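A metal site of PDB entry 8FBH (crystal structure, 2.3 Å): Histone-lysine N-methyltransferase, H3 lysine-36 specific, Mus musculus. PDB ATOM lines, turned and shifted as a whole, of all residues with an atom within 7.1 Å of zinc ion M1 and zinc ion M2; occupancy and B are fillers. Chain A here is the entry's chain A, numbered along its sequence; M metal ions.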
ATOM      1  N   ARG A  44      -7.206  15.153  -6.313  1.00  0.00           N
ATOM      2  CA  ARG A  44      -7.567  16.216  -7.290  1.00  0.00           C
ATOM      3  C   ARG A  44      -9.075  16.300  -7.382  1.00  0.00           C
ATOM      4  O   ARG A  44      -9.722  15.243  -7.581  1.00  0.00           O
ATOM      5  CB  ARG A  44      -6.968  15.944  -8.671  1.00  0.00           C
ATOM      6  CG  ARG A  44      -5.449  15.900  -8.722  1.00  0.00           C
ATOM      7  CD  ARG A  44      -5.020  15.415 -10.089  1.00  0.00           C
ATOM      8  NE  ARG A  44      -3.677  15.807 -10.490  1.00  0.00           N
ATOM      9  CZ  ARG A  44      -2.606  15.026 -10.419  1.00  0.00           C
ATOM     10  NH1 ARG A  44      -2.709  13.784  -9.950  1.00  0.00           N
ATOM     11  NH2 ARG A  44      -1.432  15.504 -10.792  1.00  0.00           N
ATOM     12  N   CYS A  45      -9.638  17.484  -7.177  1.00  0.00           N
ATOM     13  CA  CYS A  45     -11.099  17.687  -7.098  1.00  0.00           C
ATOM     14  C   CYS A  45     -11.654  17.775  -8.523  1.00  0.00           C
ATOM     15  O   CYS A  45     -10.838  17.635  -9.470  1.00  0.00           O
ATOM     16  CB  CYS A  45     -11.451  18.936  -6.289  1.00  0.00           C
ATOM     17  SG  CYS A  45     -11.024  20.477  -7.145  1.00  0.00           S
ATOM     18  N   ASN A  46     -12.972  18.017  -8.639  1.00  0.00           N
ATOM     19  CA  ASN A  46     -13.741  18.086  -9.895  1.00  0.00           C
ATOM     20  C   ASN A  46     -13.873  19.538 -10.373  1.00  0.00           C
ATOM     21  O   ASN A  46     -14.477  19.731 -11.406  1.00  0.00           O
ATOM     22  CB  ASN A  46     -15.143  17.482  -9.716  1.00  0.00           C
ATOM     23  CG  ASN A  46     -15.862  17.980  -8.482  1.00  0.00           C
ATOM     24  OD1 ASN A  46     -15.229  18.217  -7.457  1.00  0.00           O
ATOM     25  ND2 ASN A  46     -17.178  18.114  -8.569  1.00  0.00           N
ATOM     26  N   CYS A  47     -13.311  20.504  -9.665  1.00  0.00           N
ATOM     27  CA  CYS A  47     -13.402  21.959 -10.026  1.00  0.00           C
ATOM     28  C   CYS A  47     -12.468  22.274 -11.197  1.00  0.00           C
ATOM     29  O   CYS A  47     -11.460  21.548 -11.394  1.00  0.00           O
ATOM     30  CB  CYS A  47     -13.091  22.865  -8.836  1.00  0.00           C
ATOM     31  SG  CYS A  47     -14.166  22.613  -7.394  1.00  0.00           S
ATOM     32  N   LYS A  48     -12.795  23.335 -11.948  1.00  0.00           N
ATOM     33  CA  LYS A  48     -12.013  23.840 -13.125  1.00  0.00           C
ATOM     34  C   LYS A  48     -11.680  25.321 -12.927  1.00  0.00           C
ATOM     35  O   LYS A  48     -12.517  26.049 -12.332  1.00  0.00           O
ATOM     36  CB  LYS A  48     -12.833  23.677 -14.418  1.00  0.00           C
ATOM     37  CG  LYS A  48     -13.266  22.255 -14.777  1.00  0.00           C
ATOM     38  CD  LYS A  48     -12.109  21.246 -14.901  1.00  0.00           C
ATOM     39  CE  LYS A  48     -12.545  19.837 -15.277  1.00  0.00           C
ATOM     40  NZ  LYS A  48     -13.092  19.065 -14.126  1.00  0.00           N
ATOM     41  N   ASP A  51     -14.524  27.762 -13.702  1.00  0.00           N
ATOM     42  CA  ASP A  51     -15.741  27.776 -12.830  1.00  0.00           C
ATOM     43  C   ASP A  51     -15.834  29.184 -12.217  1.00  0.00           C
ATOM     44  O   ASP A  51     -14.820  29.914 -12.312  1.00  0.00           O
ATOM     45  CB  ASP A  51     -15.731  26.675 -11.765  1.00  0.00           C
ATOM     46  CG  ASP A  51     -15.921  25.243 -12.286  1.00  0.00           C
ATOM     47  OD1 ASP A  51     -16.275  25.060 -13.460  1.00  0.00           O
ATOM     48  OD2 ASP A  51     -15.703  24.305 -11.505  1.00  0.00           O
ATOM     49  N   ASN A  53     -16.493  30.167  -8.922  1.00  0.00           N
ATOM     50  CA  ASN A  53     -15.740  30.161  -7.646  1.00  0.00           C
ATOM     51  C   ASN A  53     -15.121  28.787  -7.441  1.00  0.00           C
ATOM     52  O   ASN A  53     -15.598  27.980  -6.629  1.00  0.00           O
ATOM     53  CB  ASN A  53     -16.623  30.537  -6.453  1.00  0.00           C
ATOM     54  CG  ASN A  53     -17.024  31.989  -6.473  1.00  0.00           C
ATOM     55  OD1 ASN A  53     -16.168  32.860  -6.380  1.00  0.00           O
ATOM     56  ND2 ASN A  53     -18.312  32.269  -6.611  1.00  0.00           N
ATOM     57  N   PRO A  54     -14.010  28.490  -8.140  1.00  0.00           N
ATOM     58  CA  PRO A  54     -13.364  27.196  -8.021  1.00  0.00           C
ATOM     59  C   PRO A  54     -13.098  26.823  -6.549  1.00  0.00           C
ATOM     60  O   PRO A  54     -12.461  27.606  -5.842  1.00  0.00           O
ATOM     61  CB  PRO A  54     -12.037  27.347  -8.783  1.00  0.00           C
ATOM     62  CG  PRO A  54     -12.193  28.581  -9.623  1.00  0.00           C
ATOM     63  CD  PRO A  54     -13.238  29.437  -8.947  1.00  0.00           C
ATOM     64  N   CYS A  55     -13.635  25.673  -6.108  1.00  0.00           N
ATOM     65  CA  CYS A  55     -13.386  25.057  -4.781  1.00  0.00           C
ATOM     66  C   CYS A  55     -13.991  25.941  -3.656  1.00  0.00           C
ATOM     67  O   CYS A  55     -13.632  25.770  -2.478  1.00  0.00           O
ATOM     68  CB  CYS A  55     -11.881  24.791  -4.579  1.00  0.00           C
ATOM     69  SG  CYS A  55     -11.083  23.856  -5.925  1.00  0.00           S
ATOM     70  N   GLY A  56     -14.956  26.790  -3.980  1.00  0.00           N
ATOM     71  CA  GLY A  56     -15.600  27.696  -3.009  1.00  0.00           C
ATOM     72  C   GLY A  56     -16.672  26.998  -2.171  1.00  0.00           C
ATOM     73  O   GLY A  56     -17.045  25.841  -2.521  1.00  0.00           O
ATOM     74  N   SER A  59     -19.467  25.761  -4.295  1.00  0.00           N
ATOM     75  CA  SER A  59     -19.103  24.933  -5.494  1.00  0.00           C
ATOM     76  C   SER A  59     -19.442  23.446  -5.243  1.00  0.00           C
ATOM     77  O   SER A  59     -19.820  23.085  -4.115  1.00  0.00           O
ATOM     78  CB  SER A  59     -17.648  25.086  -5.856  1.00  0.00           C
ATOM     79  OG  SER A  59     -16.823  24.457  -4.872  1.00  0.00           O
ATOM     80  N   GLU A  60     -19.242  22.628  -6.271  1.00  0.00           N
ATOM     81  CA  GLU A  60     -19.493  21.171  -6.276  1.00  0.00           C
ATOM     82  C   GLU A  60     -18.257  20.409  -5.769  1.00  0.00           C
ATOM     83  O   GLU A  60     -18.259  19.139  -5.798  1.00  0.00           O
ATOM     84  CB  GLU A  60     -19.877  20.753  -7.697  1.00  0.00           C
ATOM     85  CG  GLU A  60     -21.100  21.488  -8.245  1.00  0.00           C
ATOM     86  CD  GLU A  60     -21.401  21.237  -9.729  1.00  0.00           C
ATOM     87  OE1 GLU A  60     -22.501  21.606 -10.173  1.00  0.00           O
ATOM     88  OE2 GLU A  60     -20.526  20.642 -10.434  1.00  0.00           O
ATOM     89  N   CYS A  61     -17.254  21.144  -5.282  1.00  0.00           N
ATOM     90  CA  CYS A  61     -15.878  20.628  -4.957  1.00  0.00           C
ATOM     91  C   CYS A  61     -15.933  19.417  -4.024  1.00  0.00           C
ATOM     92  O   CYS A  61     -16.287  19.593  -2.847  1.00  0.00           O
ATOM     93  CB  CYS A  61     -15.028  21.698  -4.271  1.00  0.00           C
ATOM     94  SG  CYS A  61     -13.304  21.194  -4.126  1.00  0.00           S
ATOM     95  N   ILE A  62     -15.451  18.264  -4.508  1.00  0.00           N
ATOM     96  CA  ILE A  62     -15.413  16.984  -3.738  1.00  0.00           C
ATOM     97  C   ILE A  62     -14.397  17.085  -2.594  1.00  0.00           C
ATOM     98  O   ILE A  62     -14.616  16.397  -1.590  1.00  0.00           O
ATOM     99  CB  ILE A  62     -15.140  15.789  -4.649  1.00  0.00           C
ATOM    100  CG1 ILE A  62     -15.430  14.468  -3.936  1.00  0.00           C
ATOM    101  CG2 ILE A  62     -13.718  15.802  -5.192  1.00  0.00           C
ATOM    102  CD1 ILE A  62     -16.879  14.299  -3.548  1.00  0.00           C
ATOM    103  N   ASN A  63     -13.304  17.838  -2.752  1.00  0.00           N
ATOM    104  CA  ASN A  63     -12.309  17.982  -1.656  1.00  0.00           C
ATOM    105  C   ASN A  63     -13.010  18.636  -0.447  1.00  0.00           C
ATOM    106  O   ASN A  63     -12.978  18.061   0.667  1.00  0.00           O
ATOM    107  CB  ASN A  63     -11.018  18.668  -2.136  1.00  0.00           C
ATOM    108  CG  ASN A  63     -10.082  17.720  -2.864  1.00  0.00           C
ATOM    109  OD1 ASN A  63     -10.357  16.508  -2.935  1.00  0.00           O
ATOM    110  ND2 ASN A  63      -9.004  18.242  -3.444  1.00  0.00           N
ATOM    111  N   ARG A  64     -13.649  19.788  -0.663  1.00  0.00           N
ATOM    112  CA  ARG A  64     -14.327  20.552   0.404  1.00  0.00           C
ATOM    113  C   ARG A  64     -15.463  19.674   0.963  1.00  0.00           C
ATOM    114  O   ARG A  64     -15.586  19.604   2.185  1.00  0.00           O
ATOM    115  CB  ARG A  64     -14.746  21.919  -0.176  1.00  0.00           C
ATOM    116  CG  ARG A  64     -15.775  22.691   0.616  1.00  0.00           C
ATOM    117  CD  ARG A  64     -16.154  23.992  -0.065  1.00  0.00           C
ATOM    118  NE  ARG A  64     -15.069  24.962  -0.075  1.00  0.00           N
ATOM    119  CZ  ARG A  64     -14.659  25.649   0.981  1.00  0.00           C
ATOM    120  NH1 ARG A  64     -15.235  25.471   2.158  1.00  0.00           N
ATOM    121  NH2 ARG A  64     -13.669  26.521   0.872  1.00  0.00           N
ATOM    122  N   GLU A  69      -8.516  19.857   2.316  1.00  0.00           N
ATOM    123  CA  GLU A  69      -7.939  21.094   1.731  1.00  0.00           C
ATOM    124  C   GLU A  69      -7.162  20.725   0.444  1.00  0.00           C
ATOM    125  O   GLU A  69      -6.465  19.700   0.426  1.00  0.00           O
ATOM    126  CB  GLU A  69      -7.078  21.782   2.787  1.00  0.00           C
ATOM    127  CG  GLU A  69      -6.307  22.959   2.236  1.00  0.00           C
ATOM    128  CD  GLU A  69      -6.041  24.083   3.221  1.00  0.00           C
ATOM    129  OE1 GLU A  69      -4.901  24.616   3.214  1.00  0.00           O
ATOM    130  OE2 GLU A  69      -6.978  24.473   3.941  1.00  0.00           O
ATOM    131  N   CYS A  70      -7.286  21.536  -0.587  1.00  0.00           N
ATOM    132  CA  CYS A  70      -6.500  21.398  -1.836  1.00  0.00           C
ATOM    133  C   CYS A  70      -5.031  21.764  -1.586  1.00  0.00           C
ATOM    134  O   CYS A  70      -4.776  22.641  -0.729  1.00  0.00           O
ATOM    135  CB  CYS A  70      -7.075  22.280  -2.937  1.00  0.00           C
ATOM    136  SG  CYS A  70      -8.703  21.739  -3.498  1.00  0.00           S
ATOM    137  N   HIS A  71      -4.128  21.136  -2.318  1.00  0.00           N
ATOM    138  CA  HIS A  71      -2.713  21.573  -2.443  1.00  0.00           C
ATOM    139  C   HIS A  71      -2.584  22.463  -3.684  1.00  0.00           C
ATOM    140  O   HIS A  71      -3.079  22.107  -4.746  1.00  0.00           O
ATOM    141  CB  HIS A  71      -1.750  20.371  -2.444  1.00  0.00           C
ATOM    142  CG  HIS A  71      -0.349  20.807  -2.147  1.00  0.00           C
ATOM    143  ND1 HIS A  71       0.424  21.463  -3.084  1.00  0.00           N
ATOM    144  CD2 HIS A  71       0.343  20.853  -0.980  1.00  0.00           C
ATOM    145  CE1 HIS A  71       1.565  21.827  -2.541  1.00  0.00           C
ATOM    146  NE2 HIS A  71       1.543  21.454  -1.248  1.00  0.00           N
ATOM    147  N   VAL A  74      -1.336  21.025  -6.975  1.00  0.00           N
ATOM    148  CA  VAL A  74      -2.088  19.786  -7.386  1.00  0.00           C
ATOM    149  C   VAL A  74      -3.496  20.139  -7.877  1.00  0.00           C
ATOM    150  O   VAL A  74      -3.995  19.438  -8.781  1.00  0.00           O
ATOM    151  CB  VAL A  74      -2.148  18.769  -6.226  1.00  0.00           C
ATOM    152  CG1 VAL A  74      -3.220  17.724  -6.419  1.00  0.00           C
ATOM    153  CG2 VAL A  74      -0.807  18.091  -6.012  1.00  0.00           C
ATOM    154  N   CYS A  75      -4.159  21.128  -7.278  1.00  0.00           N
ATOM    155  CA  CYS A  75      -5.543  21.492  -7.614  1.00  0.00           C
ATOM    156  C   CYS A  75      -5.611  21.983  -9.067  1.00  0.00           C
ATOM    157  O   CYS A  75      -4.909  22.899  -9.441  1.00  0.00           O
ATOM    158  CB  CYS A  75      -6.112  22.566  -6.693  1.00  0.00           C
ATOM    159  SG  CYS A  75      -7.837  22.944  -7.091  1.00  0.00           S
ATOM    160  N   PRO A  76      -6.503  21.401  -9.897  1.00  0.00           N
ATOM    161  CA  PRO A  76      -6.648  21.816 -11.289  1.00  0.00           C
ATOM    162  C   PRO A  76      -7.074  23.268 -11.472  1.00  0.00           C
ATOM    163  O   PRO A  76      -6.909  23.753 -12.560  1.00  0.00           O
ATOM    164  CB  PRO A  76      -7.791  20.935 -11.831  1.00  0.00           C
ATOM    165  CG  PRO A  76      -7.786  19.733 -10.915  1.00  0.00           C
ATOM    166  CD  PRO A  76      -7.345  20.253  -9.564  1.00  0.00           C
ATOM    167  N   ALA A  77      -7.680  23.880 -10.462  1.00  0.00           N
ATOM    168  CA  ALA A  77      -8.095  25.302 -10.473  1.00  0.00           C
ATOM    169  C   ALA A  77      -6.888  26.226 -10.231  1.00  0.00           C
ATOM    170  O   ALA A  77      -7.010  27.436 -10.499  1.00  0.00           O
ATOM    171  CB  ALA A  77      -9.171  25.520  -9.449  1.00  0.00           C
ATOM    172  N   GLY A  78      -5.753  25.666  -9.809  1.00  0.00           N
ATOM    173  CA  GLY A  78      -4.511  26.411  -9.532  1.00  0.00           C
ATOM    174  C   GLY A  78      -4.706  27.492  -8.468  1.00  0.00           C
ATOM    175  O   GLY A  78      -5.396  27.219  -7.449  1.00  0.00           O
ATOM    176  N   ARG A  80      -6.547  29.931  -8.484  1.00  0.00           N
ATOM    177  CA  ARG A  80      -7.970  30.331  -8.393  1.00  0.00           C
ATOM    178  C   ARG A  80      -8.700  29.496  -7.306  1.00  0.00           C
ATOM    179  O   ARG A  80      -9.860  29.867  -6.939  1.00  0.00           O
ATOM    180  CB  ARG A  80      -8.623  30.269  -9.779  1.00  0.00           C
ATOM    181  CG  ARG A  80      -8.151  31.406 -10.707  1.00  0.00           C
ATOM    182  CD  ARG A  80      -8.928  31.628 -12.002  1.00  0.00           C
ATOM    183  NE  ARG A  80     -10.334  31.234 -11.966  1.00  0.00           N
ATOM    184  CZ  ARG A  80     -11.355  31.928 -11.419  1.00  0.00           C
ATOM    185  NH1 ARG A  80     -12.586  31.438 -11.481  1.00  0.00           N
ATOM    186  NH2 ARG A  80     -11.141  33.082 -10.818  1.00  0.00           N
ATOM    187  N   CYS A  81      -8.008  28.484  -6.731  1.00  0.00           N
ATOM    188  CA  CYS A  81      -8.505  27.577  -5.647  1.00  0.00           C
ATOM    189  C   CYS A  81      -8.934  28.371  -4.404  1.00  0.00           C
ATOM    190  O   CYS A  81      -8.073  28.974  -3.795  1.00  0.00           O
ATOM    191  CB  CYS A  81      -7.435  26.586  -5.227  1.00  0.00           C
ATOM    192  SG  CYS A  81      -8.016  25.298  -4.107  1.00  0.00           S
ATOM    193  N   GLN A  82     -10.216  28.298  -4.013  1.00  0.00           N
ATOM    194  CA  GLN A  82     -10.784  28.951  -2.791  1.00  0.00           C
ATOM    195  C   GLN A  82     -10.899  27.936  -1.635  1.00  0.00           C
ATOM    196  O   GLN A  82     -11.743  28.154  -0.747  1.00  0.00           O
ATOM    197  CB  GLN A  82     -12.155  29.532  -3.136  1.00  0.00           C
ATOM    198  CG  GLN A  82     -12.112  30.683  -4.131  1.00  0.00           C
ATOM    199  CD  GLN A  82     -13.499  31.208  -4.430  1.00  0.00           C
ATOM    200  OE1 GLN A  82     -14.461  30.949  -3.709  1.00  0.00           O
ATOM    201  NE2 GLN A  82     -13.619  31.936  -5.535  1.00  0.00           N
ATOM    202  N   ASN A  83     -10.103  26.858  -1.654  1.00  0.00           N
ATOM    203  CA  ASN A  83     -10.139  25.757  -0.659  1.00  0.00           C
ATOM    204  C   ASN A  83      -8.748  25.595  -0.034  1.00  0.00           C
ATOM    205  O   ASN A  83      -8.266  24.443   0.007  1.00  0.00           O
ATOM    206  CB  ASN A  83     -10.639  24.451  -1.270  1.00  0.00           C
ATOM    207  CG  ASN A  83     -10.902  23.374  -0.233  1.00  0.00           C
ATOM    208  OD1 ASN A  83     -11.199  23.709   0.909  1.00  0.00           O
ATOM    209  ND2 ASN A  83     -10.785  22.120  -0.605  1.00  0.00           N
ATOM    210  N   GLN A  84      -8.128  26.688   0.439  1.00  0.00           N
ATOM    211  CA  GLN A  84      -6.783  26.669   1.079  1.00  0.00           C
ATOM    212  C   GLN A  84      -6.811  27.499   2.377  1.00  0.00           C
ATOM    213  O   GLN A  84      -5.778  28.118   2.701  1.00  0.00           O
ATOM    214  CB  GLN A  84      -5.729  27.176   0.096  1.00  0.00           C
ATOM    215  CG  GLN A  84      -5.464  26.193  -1.032  1.00  0.00           C
ATOM    216  CD  GLN A  84      -4.644  26.765  -2.163  1.00  0.00           C
ATOM    217  OE1 GLN A  84      -4.965  26.584  -3.336  1.00  0.00           O
ATOM    218  NE2 GLN A  84      -3.547  27.420  -1.829  1.00  0.00           N
HETATM  219 ZN    ZN M   1     -12.325  21.943  -6.026  1.00  0.00          ZN
HETATM  220 ZN    ZN M   2      -8.992  23.393  -5.112  1.00  0.00          ZN
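The side-chain sulfur (SG) of Cys 61 sits close to the backbone NH (N) of Asn 63, at 3.6 Å. OG of Ser 59 lies close to N of Cys 61. The backbone NH of Arg 64 lies close to the side-chain sulfur of Cys 61, 3.8 Å away. O of Cys 55 lies within hydrogen-bond range of NE of Arg 64, at 2.9 Å. N of Cys 70 sits at hydrogen-bond distance from O of Asn 83, at 3.1 Å. SG of Cys 70 sits close to ND2 of Asn 63 (3.5 Å). SG of Cys 75 lies close to N of Ala 77 (3.5 Å). SG of Cys 81 sits close to N of Asn 83, 3.6 Å away.
Of the 29 residues printed, 4 come within 4 Å of zinc ion M1. The nearest printed residue that does not touch zinc ion M1 is Cys 70 (4.4 Å).
Within 4 Å of zinc ion M2: Cys 55, Cys 70, Cys 75 and Cys 81. The nearest printed residue that does not touch zinc ion M2 is Cys 45 (4.1 Å).
Zinc ion M1 is bound by SG of Cys 45 (2.3 Å), SG of Cys 61 (2.3 Å), SG of Cys 55 (2.3 Å) and SG of Cys 47 (2.4 Å). Zinc ion M1 has four donor atoms within binding distance.
Zinc ion M2 is bound by SG of Cys 55 (2.3 Å), SG of Cys 70 (2.3 Å), SG of Cys 75 (2.3 Å) and SG of Cys 81 (2.4 Å).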
